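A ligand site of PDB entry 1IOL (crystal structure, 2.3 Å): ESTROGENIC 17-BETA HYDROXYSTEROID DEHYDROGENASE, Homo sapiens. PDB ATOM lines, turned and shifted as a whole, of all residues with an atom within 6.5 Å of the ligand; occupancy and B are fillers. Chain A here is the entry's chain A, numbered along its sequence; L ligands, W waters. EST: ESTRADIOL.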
ATOM      1  N   GLY A 141     -13.428  -4.346   2.930  1.00  0.00           N
ATOM      2  CA  GLY A 141     -13.550  -5.750   3.259  1.00  0.00           C
ATOM      3  C   GLY A 141     -14.026  -5.905   4.681  1.00  0.00           C
ATOM      4  O   GLY A 141     -14.591  -4.990   5.276  1.00  0.00           O
ATOM      5  N   SER A 142     -13.822  -7.097   5.216  1.00  0.00           N
ATOM      6  CA  SER A 142     -14.199  -7.419   6.587  1.00  0.00           C
ATOM      7  C   SER A 142     -13.472  -8.689   6.948  1.00  0.00           C
ATOM      8  O   SER A 142     -13.170  -9.483   6.069  1.00  0.00           O
ATOM      9  CB  SER A 142     -15.691  -7.676   6.679  1.00  0.00           C
ATOM     10  OG  SER A 142     -15.992  -8.274   7.926  1.00  0.00           O
ATOM     11  N   VAL A 143     -13.139  -8.870   8.213  1.00  0.00           N
ATOM     12  CA  VAL A 143     -12.492 -10.122   8.582  1.00  0.00           C
ATOM     13  C   VAL A 143     -13.571 -11.207   8.495  1.00  0.00           C
ATOM     14  O   VAL A 143     -13.283 -12.388   8.604  1.00  0.00           O
ATOM     15  CB  VAL A 143     -11.872 -10.078   9.975  1.00  0.00           C
ATOM     16  CG1 VAL A 143     -10.895  -8.914  10.061  1.00  0.00           C
ATOM     17  CG2 VAL A 143     -12.935  -9.976  11.037  1.00  0.00           C
ATOM     18  N   GLY A 144     -14.817 -10.779   8.317  1.00  0.00           N
ATOM     19  CA  GLY A 144     -15.912 -11.713   8.148  1.00  0.00           C
ATOM     20  C   GLY A 144     -15.867 -12.214   6.705  1.00  0.00           C
ATOM     21  O   GLY A 144     -16.720 -12.964   6.255  1.00  0.00           O
ATOM     22  N   GLY A 145     -14.899 -11.710   5.951  1.00  0.00           N
ATOM     23  CA  GLY A 145     -14.718 -12.140   4.585  1.00  0.00           C
ATOM     24  C   GLY A 145     -13.498 -13.038   4.534  1.00  0.00           C
ATOM     25  O   GLY A 145     -13.157 -13.543   3.478  1.00  0.00           O
ATOM     26  N   MET A 147     -12.990 -15.374   7.425  1.00  0.00           N
ATOM     27  CA  MET A 147     -13.349 -16.487   8.289  1.00  0.00           C
ATOM     28  C   MET A 147     -14.865 -16.445   8.483  1.00  0.00           C
ATOM     29  O   MET A 147     -15.456 -15.373   8.451  1.00  0.00           O
ATOM     30  CB  MET A 147     -12.614 -16.392   9.622  1.00  0.00           C
ATOM     31  CG  MET A 147     -12.949 -15.171  10.468  1.00  0.00           C
ATOM     32  SD  MET A 147     -11.898 -15.075  11.913  1.00  0.00           S
ATOM     33  CE  MET A 147     -10.407 -14.607  11.129  1.00  0.00           C
ATOM     34  N   LEU A 149     -18.492 -16.737  10.370  1.00  0.00           N
ATOM     35  CA  LEU A 149     -19.009 -16.391  11.706  1.00  0.00           C
ATOM     36  C   LEU A 149     -20.441 -16.866  11.839  1.00  0.00           C
ATOM     37  O   LEU A 149     -21.271 -16.619  10.974  1.00  0.00           O
ATOM     38  CB  LEU A 149     -18.973 -14.868  11.915  1.00  0.00           C
ATOM     39  CG  LEU A 149     -17.612 -14.178  11.782  1.00  0.00           C
ATOM     40  CD1 LEU A 149     -17.792 -12.671  11.596  1.00  0.00           C
ATOM     41  CD2 LEU A 149     -16.730 -14.509  12.962  1.00  0.00           C
ATOM     42  N   ASN A 152     -24.048 -15.193  10.720  1.00  0.00           N
ATOM     43  CA  ASN A 152     -23.747 -14.183   9.694  1.00  0.00           C
ATOM     44  C   ASN A 152     -23.506 -14.866   8.346  1.00  0.00           C
ATOM     45  O   ASN A 152     -22.837 -14.312   7.480  1.00  0.00           O
ATOM     46  CB  ASN A 152     -22.496 -13.392  10.066  1.00  0.00           C
ATOM     47  CG  ASN A 152     -22.756 -12.376  11.169  1.00  0.00           C
ATOM     48  OD1 ASN A 152     -23.326 -11.320  10.918  1.00  0.00           O
ATOM     49  ND2 ASN A 152     -22.353 -12.709  12.381  1.00  0.00           N
ATOM     50  N   TYR A 155     -23.938 -12.848   5.187  1.00  0.00           N
ATOM     51  CA  TYR A 155     -23.075 -11.689   5.242  1.00  0.00           C
ATOM     52  C   TYR A 155     -21.652 -12.123   4.863  1.00  0.00           C
ATOM     53  O   TYR A 155     -21.007 -11.472   4.037  1.00  0.00           O
ATOM     54  CB  TYR A 155     -23.095 -11.066   6.641  1.00  0.00           C
ATOM     55  CG  TYR A 155     -22.095  -9.968   6.804  1.00  0.00           C
ATOM     56  CD1 TYR A 155     -22.226  -8.773   6.121  1.00  0.00           C
ATOM     57  CD2 TYR A 155     -20.989 -10.147   7.623  1.00  0.00           C
ATOM     58  CE1 TYR A 155     -21.263  -7.782   6.242  1.00  0.00           C
ATOM     59  CE2 TYR A 155     -20.032  -9.168   7.749  1.00  0.00           C
ATOM     60  CZ  TYR A 155     -20.174  -7.989   7.055  1.00  0.00           C
ATOM     61  OH  TYR A 155     -19.215  -7.025   7.189  1.00  0.00           O
ATOM     62  N   CYS A 156     -21.177 -13.209   5.481  1.00  0.00           N
ATOM     63  CA  CYS A 156     -19.835 -13.745   5.203  1.00  0.00           C
ATOM     64  C   CYS A 156     -19.753 -14.241   3.760  1.00  0.00           C
ATOM     65  O   CYS A 156     -18.698 -14.190   3.146  1.00  0.00           O
ATOM     66  CB  CYS A 156     -19.504 -14.885   6.152  1.00  0.00           C
ATOM     67  SG  CYS A 156     -19.420 -14.389   7.848  1.00  0.00           S
ATOM     68  N   CYS A 185     -11.510  -4.638   7.661  1.00  0.00           N
ATOM     69  CA  CYS A 185     -11.952  -4.043   8.913  1.00  0.00           C
ATOM     70  C   CYS A 185     -12.444  -5.063   9.920  1.00  0.00           C
ATOM     71  O   CYS A 185     -13.036  -6.088   9.562  1.00  0.00           O
ATOM     72  CB  CYS A 185     -13.131  -3.078   8.661  1.00  0.00           C
ATOM     73  SG  CYS A 185     -12.925  -1.980   7.295  1.00  0.00           S
ATOM     74  N   GLY A 186     -12.184  -4.773  11.190  1.00  0.00           N
ATOM     75  CA  GLY A 186     -12.674  -5.614  12.264  1.00  0.00           C
ATOM     76  C   GLY A 186     -13.911  -4.799  12.652  1.00  0.00           C
ATOM     77  O   GLY A 186     -14.474  -4.105  11.791  1.00  0.00           O
ATOM     78  N   PRO A 187     -14.366  -4.869  13.897  1.00  0.00           N
ATOM     79  CA  PRO A 187     -15.543  -4.084  14.286  1.00  0.00           C
ATOM     80  C   PRO A 187     -15.169  -2.604  14.488  1.00  0.00           C
ATOM     81  O   PRO A 187     -14.108  -2.286  15.036  1.00  0.00           O
ATOM     82  CB  PRO A 187     -15.966  -4.754  15.595  1.00  0.00           C
ATOM     83  CG  PRO A 187     -14.651  -5.192  16.171  1.00  0.00           C
ATOM     84  CD  PRO A 187     -13.945  -5.780  14.979  1.00  0.00           C
ATOM     85  N   VAL A 188     -16.003  -1.698  13.989  1.00  0.00           N
ATOM     86  CA  VAL A 188     -15.736  -0.279  14.133  1.00  0.00           C
ATOM     87  C   VAL A 188     -16.879   0.332  14.908  1.00  0.00           C
ATOM     88  O   VAL A 188     -18.040   0.019  14.662  1.00  0.00           O
ATOM     89  CB  VAL A 188     -15.583   0.429  12.761  1.00  0.00           C
ATOM     90  CG1 VAL A 188     -14.420  -0.169  12.001  1.00  0.00           C
ATOM     91  CG2 VAL A 188     -16.853   0.325  11.952  1.00  0.00           C
ATOM     92  N   MET A 193     -24.728  -0.382  15.304  1.00  0.00           N
ATOM     93  CA  MET A 193     -24.343  -1.785  15.114  1.00  0.00           C
ATOM     94  C   MET A 193     -24.767  -2.637  16.307  1.00  0.00           C
ATOM     95  O   MET A 193     -25.466  -3.642  16.133  1.00  0.00           O
ATOM     96  CB  MET A 193     -22.826  -1.918  14.906  1.00  0.00           C
ATOM     97  CG  MET A 193     -22.370  -3.334  14.586  1.00  0.00           C
ATOM     98  SD  MET A 193     -20.572  -3.524  14.429  1.00  0.00           S
ATOM     99  CE  MET A 193     -20.344  -5.176  15.090  1.00  0.00           C
ATOM    100  N   TYR A 218     -24.599 -15.977  20.935  1.00  0.00           N
ATOM    101  CA  TYR A 218     -23.756 -15.296  19.959  1.00  0.00           C
ATOM    102  C   TYR A 218     -23.838 -13.790  20.140  1.00  0.00           C
ATOM    103  O   TYR A 218     -22.837 -13.088  20.017  1.00  0.00           O
ATOM    104  CB  TYR A 218     -24.129 -15.656  18.518  1.00  0.00           C
ATOM    105  CG  TYR A 218     -23.433 -14.759  17.509  1.00  0.00           C
ATOM    106  CD1 TYR A 218     -22.056 -14.864  17.275  1.00  0.00           C
ATOM    107  CD2 TYR A 218     -24.124 -13.742  16.863  1.00  0.00           C
ATOM    108  CE1 TYR A 218     -21.400 -13.957  16.449  1.00  0.00           C
ATOM    109  CE2 TYR A 218     -23.484 -12.853  16.035  1.00  0.00           C
ATOM    110  CZ  TYR A 218     -22.124 -12.949  15.842  1.00  0.00           C
ATOM    111  OH  TYR A 218     -21.481 -12.006  15.067  1.00  0.00           O
ATOM    112  N   HIS A 221     -21.808 -12.678  23.161  1.00  0.00           N
ATOM    113  CA  HIS A 221     -20.395 -12.718  22.800  1.00  0.00           C
ATOM    114  C   HIS A 221     -20.005 -11.583  21.840  1.00  0.00           C
ATOM    115  O   HIS A 221     -18.910 -11.020  21.933  1.00  0.00           O
ATOM    116  CB  HIS A 221     -20.066 -14.079  22.184  1.00  0.00           C
ATOM    117  CG  HIS A 221     -18.703 -14.155  21.568  1.00  0.00           C
ATOM    118  ND1 HIS A 221     -18.492 -13.992  20.220  1.00  0.00           N
ATOM    119  CD2 HIS A 221     -17.492 -14.367  22.127  1.00  0.00           C
ATOM    120  CE1 HIS A 221     -17.198 -14.108  19.959  1.00  0.00           C
ATOM    121  NE2 HIS A 221     -16.569 -14.338  21.106  1.00  0.00           N
ATOM    122  N   SER A 222     -20.897 -11.286  20.919  1.00  0.00           N
ATOM    123  CA  SER A 222     -20.681 -10.235  19.928  1.00  0.00           C
ATOM    124  C   SER A 222     -20.519  -8.883  20.625  1.00  0.00           C
ATOM    125  O   SER A 222     -19.616  -8.112  20.297  1.00  0.00           O
ATOM    126  CB  SER A 222     -21.854 -10.223  18.948  1.00  0.00           C
ATOM    127  OG  SER A 222     -21.688  -9.246  17.941  1.00  0.00           O
ATOM    128  N   VAL A 225     -16.935  -8.532  22.214  1.00  0.00           N
ATOM    129  CA  VAL A 225     -15.885  -8.264  21.232  1.00  0.00           C
ATOM    130  C   VAL A 225     -15.946  -6.807  20.742  1.00  0.00           C
ATOM    131  O   VAL A 225     -14.926  -6.135  20.632  1.00  0.00           O
ATOM    132  CB  VAL A 225     -16.007  -9.230  20.018  1.00  0.00           C
ATOM    133  CG1 VAL A 225     -14.877  -9.005  19.034  1.00  0.00           C
ATOM    134  CG2 VAL A 225     -16.007 -10.666  20.503  1.00  0.00           C
ATOM    135  N   PHE A 226     -17.153  -6.327  20.470  1.00  0.00           N
ATOM    136  CA  PHE A 226     -17.345  -4.976  19.991  1.00  0.00           C
ATOM    137  C   PHE A 226     -16.839  -3.975  21.009  1.00  0.00           C
ATOM    138  O   PHE A 226     -16.080  -3.069  20.686  1.00  0.00           O
ATOM    139  CB  PHE A 226     -18.820  -4.712  19.701  1.00  0.00           C
ATOM    140  CG  PHE A 226     -19.060  -3.492  18.878  1.00  0.00           C
ATOM    141  CD1 PHE A 226     -18.700  -3.461  17.541  1.00  0.00           C
ATOM    142  CD2 PHE A 226     -19.645  -2.358  19.443  1.00  0.00           C
ATOM    143  CE1 PHE A 226     -18.911  -2.329  16.768  1.00  0.00           C
ATOM    144  CE2 PHE A 226     -19.864  -1.213  18.670  1.00  0.00           C
ATOM    145  CZ  PHE A 226     -19.496  -1.195  17.334  1.00  0.00           C
ATOM    146  N   PHE A 259      -7.105 -10.084  15.055  1.00  0.00           N
ATOM    147  CA  PHE A 259      -7.748 -11.260  14.490  1.00  0.00           C
ATOM    148  C   PHE A 259      -6.843 -12.131  13.629  1.00  0.00           C
ATOM    149  O   PHE A 259      -7.264 -13.167  13.127  1.00  0.00           O
ATOM    150  CB  PHE A 259      -9.008 -10.850  13.711  1.00  0.00           C
ATOM    151  CG  PHE A 259     -10.088 -10.236  14.572  1.00  0.00           C
ATOM    152  CD1 PHE A 259     -10.754 -11.009  15.529  1.00  0.00           C
ATOM    153  CD2 PHE A 259     -10.441  -8.898  14.438  1.00  0.00           C
ATOM    154  CE1 PHE A 259     -11.764 -10.447  16.331  1.00  0.00           C
ATOM    155  CE2 PHE A 259     -11.446  -8.334  15.231  1.00  0.00           C
ATOM    156  CZ  PHE A 259     -12.107  -9.104  16.180  1.00  0.00           C
ATOM    157  N   LEU A 262      -6.196 -16.064  14.834  1.00  0.00           N
ATOM    158  CA  LEU A 262      -7.354 -16.901  14.550  1.00  0.00           C
ATOM    159  C   LEU A 262      -7.450 -17.243  13.049  1.00  0.00           C
ATOM    160  O   LEU A 262      -8.036 -18.258  12.662  1.00  0.00           O
ATOM    161  CB  LEU A 262      -8.598 -16.168  15.040  1.00  0.00           C
ATOM    162  CG  LEU A 262      -9.988 -16.778  15.144  1.00  0.00           C
ATOM    163  CD1 LEU A 262      -9.970 -18.106  15.877  1.00  0.00           C
ATOM    164  CD2 LEU A 262     -10.858 -15.776  15.875  1.00  0.00           C
ATOM    165  N   MET A 279     -13.588 -21.742  16.885  1.00  0.00           N
ATOM    166  CA  MET A 279     -14.598 -20.696  16.816  1.00  0.00           C
ATOM    167  C   MET A 279     -15.877 -21.069  17.560  1.00  0.00           C
ATOM    168  O   MET A 279     -16.557 -20.202  18.097  1.00  0.00           O
ATOM    169  CB  MET A 279     -14.899 -20.348  15.358  1.00  0.00           C
ATOM    170  CG  MET A 279     -15.872 -19.195  15.164  1.00  0.00           C
ATOM    171  SD  MET A 279     -15.342 -17.685  15.968  1.00  0.00           S
ATOM    172  CE  MET A 279     -13.742 -17.477  15.290  1.00  0.00           C
ATOM    173  N   GLU A 282     -15.136 -20.740  21.386  1.00  0.00           N
ATOM    174  CA  GLU A 282     -15.008 -19.335  21.756  1.00  0.00           C
ATOM    175  C   GLU A 282     -16.323 -18.583  21.743  1.00  0.00           C
ATOM    176  O   GLU A 282     -16.519 -17.639  22.502  1.00  0.00           O
ATOM    177  CB  GLU A 282     -14.030 -18.627  20.806  1.00  0.00           C
ATOM    178  CG  GLU A 282     -13.841 -17.148  21.103  1.00  0.00           C
ATOM    179  CD  GLU A 282     -13.113 -16.421  19.989  1.00  0.00           C
ATOM    180  OE1 GLU A 282     -12.219 -17.035  19.366  1.00  0.00           O
ATOM    181  OE2 GLU A 282     -13.427 -15.230  19.749  1.00  0.00           O
ATOM    182  N   VAL A 283     -17.210 -18.956  20.825  1.00  0.00           N
ATOM    183  CA  VAL A 283     -18.497 -18.291  20.718  1.00  0.00           C
ATOM    184  C   VAL A 283     -19.622 -18.921  21.546  1.00  0.00           C
ATOM    185  O   VAL A 283     -20.626 -18.260  21.831  1.00  0.00           O
ATOM    186  CB  VAL A 283     -18.938 -18.180  19.225  1.00  0.00           C
ATOM    187  CG1 VAL A 283     -20.297 -17.487  19.097  1.00  0.00           C
ATOM    188  CG2 VAL A 283     -17.902 -17.403  18.438  1.00  0.00           C
HETATM  189  C1  EST L   1     -14.607 -11.414  15.191  1.00  0.00           C
HETATM  190  C2  EST L   1     -14.370 -12.590  15.930  1.00  0.00           C
HETATM  191  C3  EST L   1     -15.299 -13.001  16.879  1.00  0.00           C
HETATM  192  O3  EST L   1     -14.923 -13.914  17.838  1.00  0.00           O
HETATM  193  C4  EST L   1     -16.615 -12.492  16.851  1.00  0.00           C
HETATM  194  C5  EST L   1     -16.897 -11.346  16.065  1.00  0.00           C
HETATM  195  C6  EST L   1     -18.326 -10.725  16.150  1.00  0.00           C
HETATM  196  C7  EST L   1     -18.536  -9.386  15.345  1.00  0.00           C
HETATM  197  C8  EST L   1     -17.743  -9.421  14.001  1.00  0.00           C
HETATM  198  C9  EST L   1     -16.200  -9.549  14.337  1.00  0.00           C
HETATM  199  C10 EST L   1     -15.882 -10.792  15.222  1.00  0.00           C
HETATM  200  C11 EST L   1     -15.329  -9.409  13.044  1.00  0.00           C
HETATM  201  C12 EST L   1     -15.630  -8.145  12.211  1.00  0.00           C
HETATM  202  C13 EST L   1     -17.120  -8.055  11.787  1.00  0.00           C
HETATM  203  C14 EST L   1     -18.029  -8.177  13.075  1.00  0.00           C
HETATM  204  C15 EST L   1     -19.440  -7.881  12.508  1.00  0.00           C
HETATM  205  C16 EST L   1     -19.161  -6.762  11.455  1.00  0.00           C
HETATM  206  C17 EST L   1     -17.610  -6.643  11.367  1.00  0.00           C
HETATM  207  O17 EST L   1     -17.172  -6.232  10.024  1.00  0.00           O
HETATM  208  C18 EST L   1     -17.381  -9.119  10.653  1.00  0.00           C
HETATM  209  O   HOH W   1     -16.489  -3.638   9.631  1.00  0.00           O
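The side-chain carboxylate (OE2) of Glu 282 lies within hydrogen-bond range of an oxygen (O3) of the ligand (2.8 Å). An oxygen (O17) of the ligand lies within hydrogen-bond range of the side-chain hydroxyl (OG) of Ser 142 (3.2 Å).
The backbone NH of Gly 144 sits at hydrogen-bond distance from the side-chain hydroxyl of Ser 142, 2.8 Å away. The backbone carbonyl oxygen (O) of Cys 185 sits at hydrogen-bond distance from the backbone NH (N) of Val 143 (3.1 Å). The side-chain hydroxyl of Tyr 218 sits at hydrogen-bond distance from the side-chain amide nitrogen of Asn 152 (2.9 Å). The backbone NH (N) of Leu 149 lies within hydrogen-bond range of the side-chain sulfur (SG) of Cys 156 (3.6 Å). The backbone carbonyl oxygen (O) of Gly 144 lies close to the side-chain sulfur (SG) of Cys 156, at 3.4 Å.
Val 143 touches the ligand (CG2 to C11, 3.2 Å). N of Gly 144 touches C18 of the ligand, at 3.8 Å. Leu 149 touches the ligand (CD1 to C18, 3.7 Å). Tyr 155 touches the ligand (OH to O17, 3.6 Å). Gly 186 touches the ligand. Pro 187 touches the ligand (N to C12, 3.9 Å). Met 193 touches the ligand (CE to C15, 3.8 Å). Tyr 218 touches the ligand. CE1 of His 221 touches O3 of the ligand (3.1 Å). Phe 259 touches the ligand (CE1 to C1, 3.2 Å). Hydrophobic or aromatic side chains within 4 Å of the ligand: Val 143, Leu 149, Tyr 155, Met 193, His 221 and Phe 259. Of the 25 residues printed, 12 come within 4 Å of the ligand. The nearest printed residue that does not touch the ligand is Ser 222 (4.1 Å).
Water W1 bridges O17 of the ligand (2.7 Å) and O of Gly 186 (3.0 Å).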
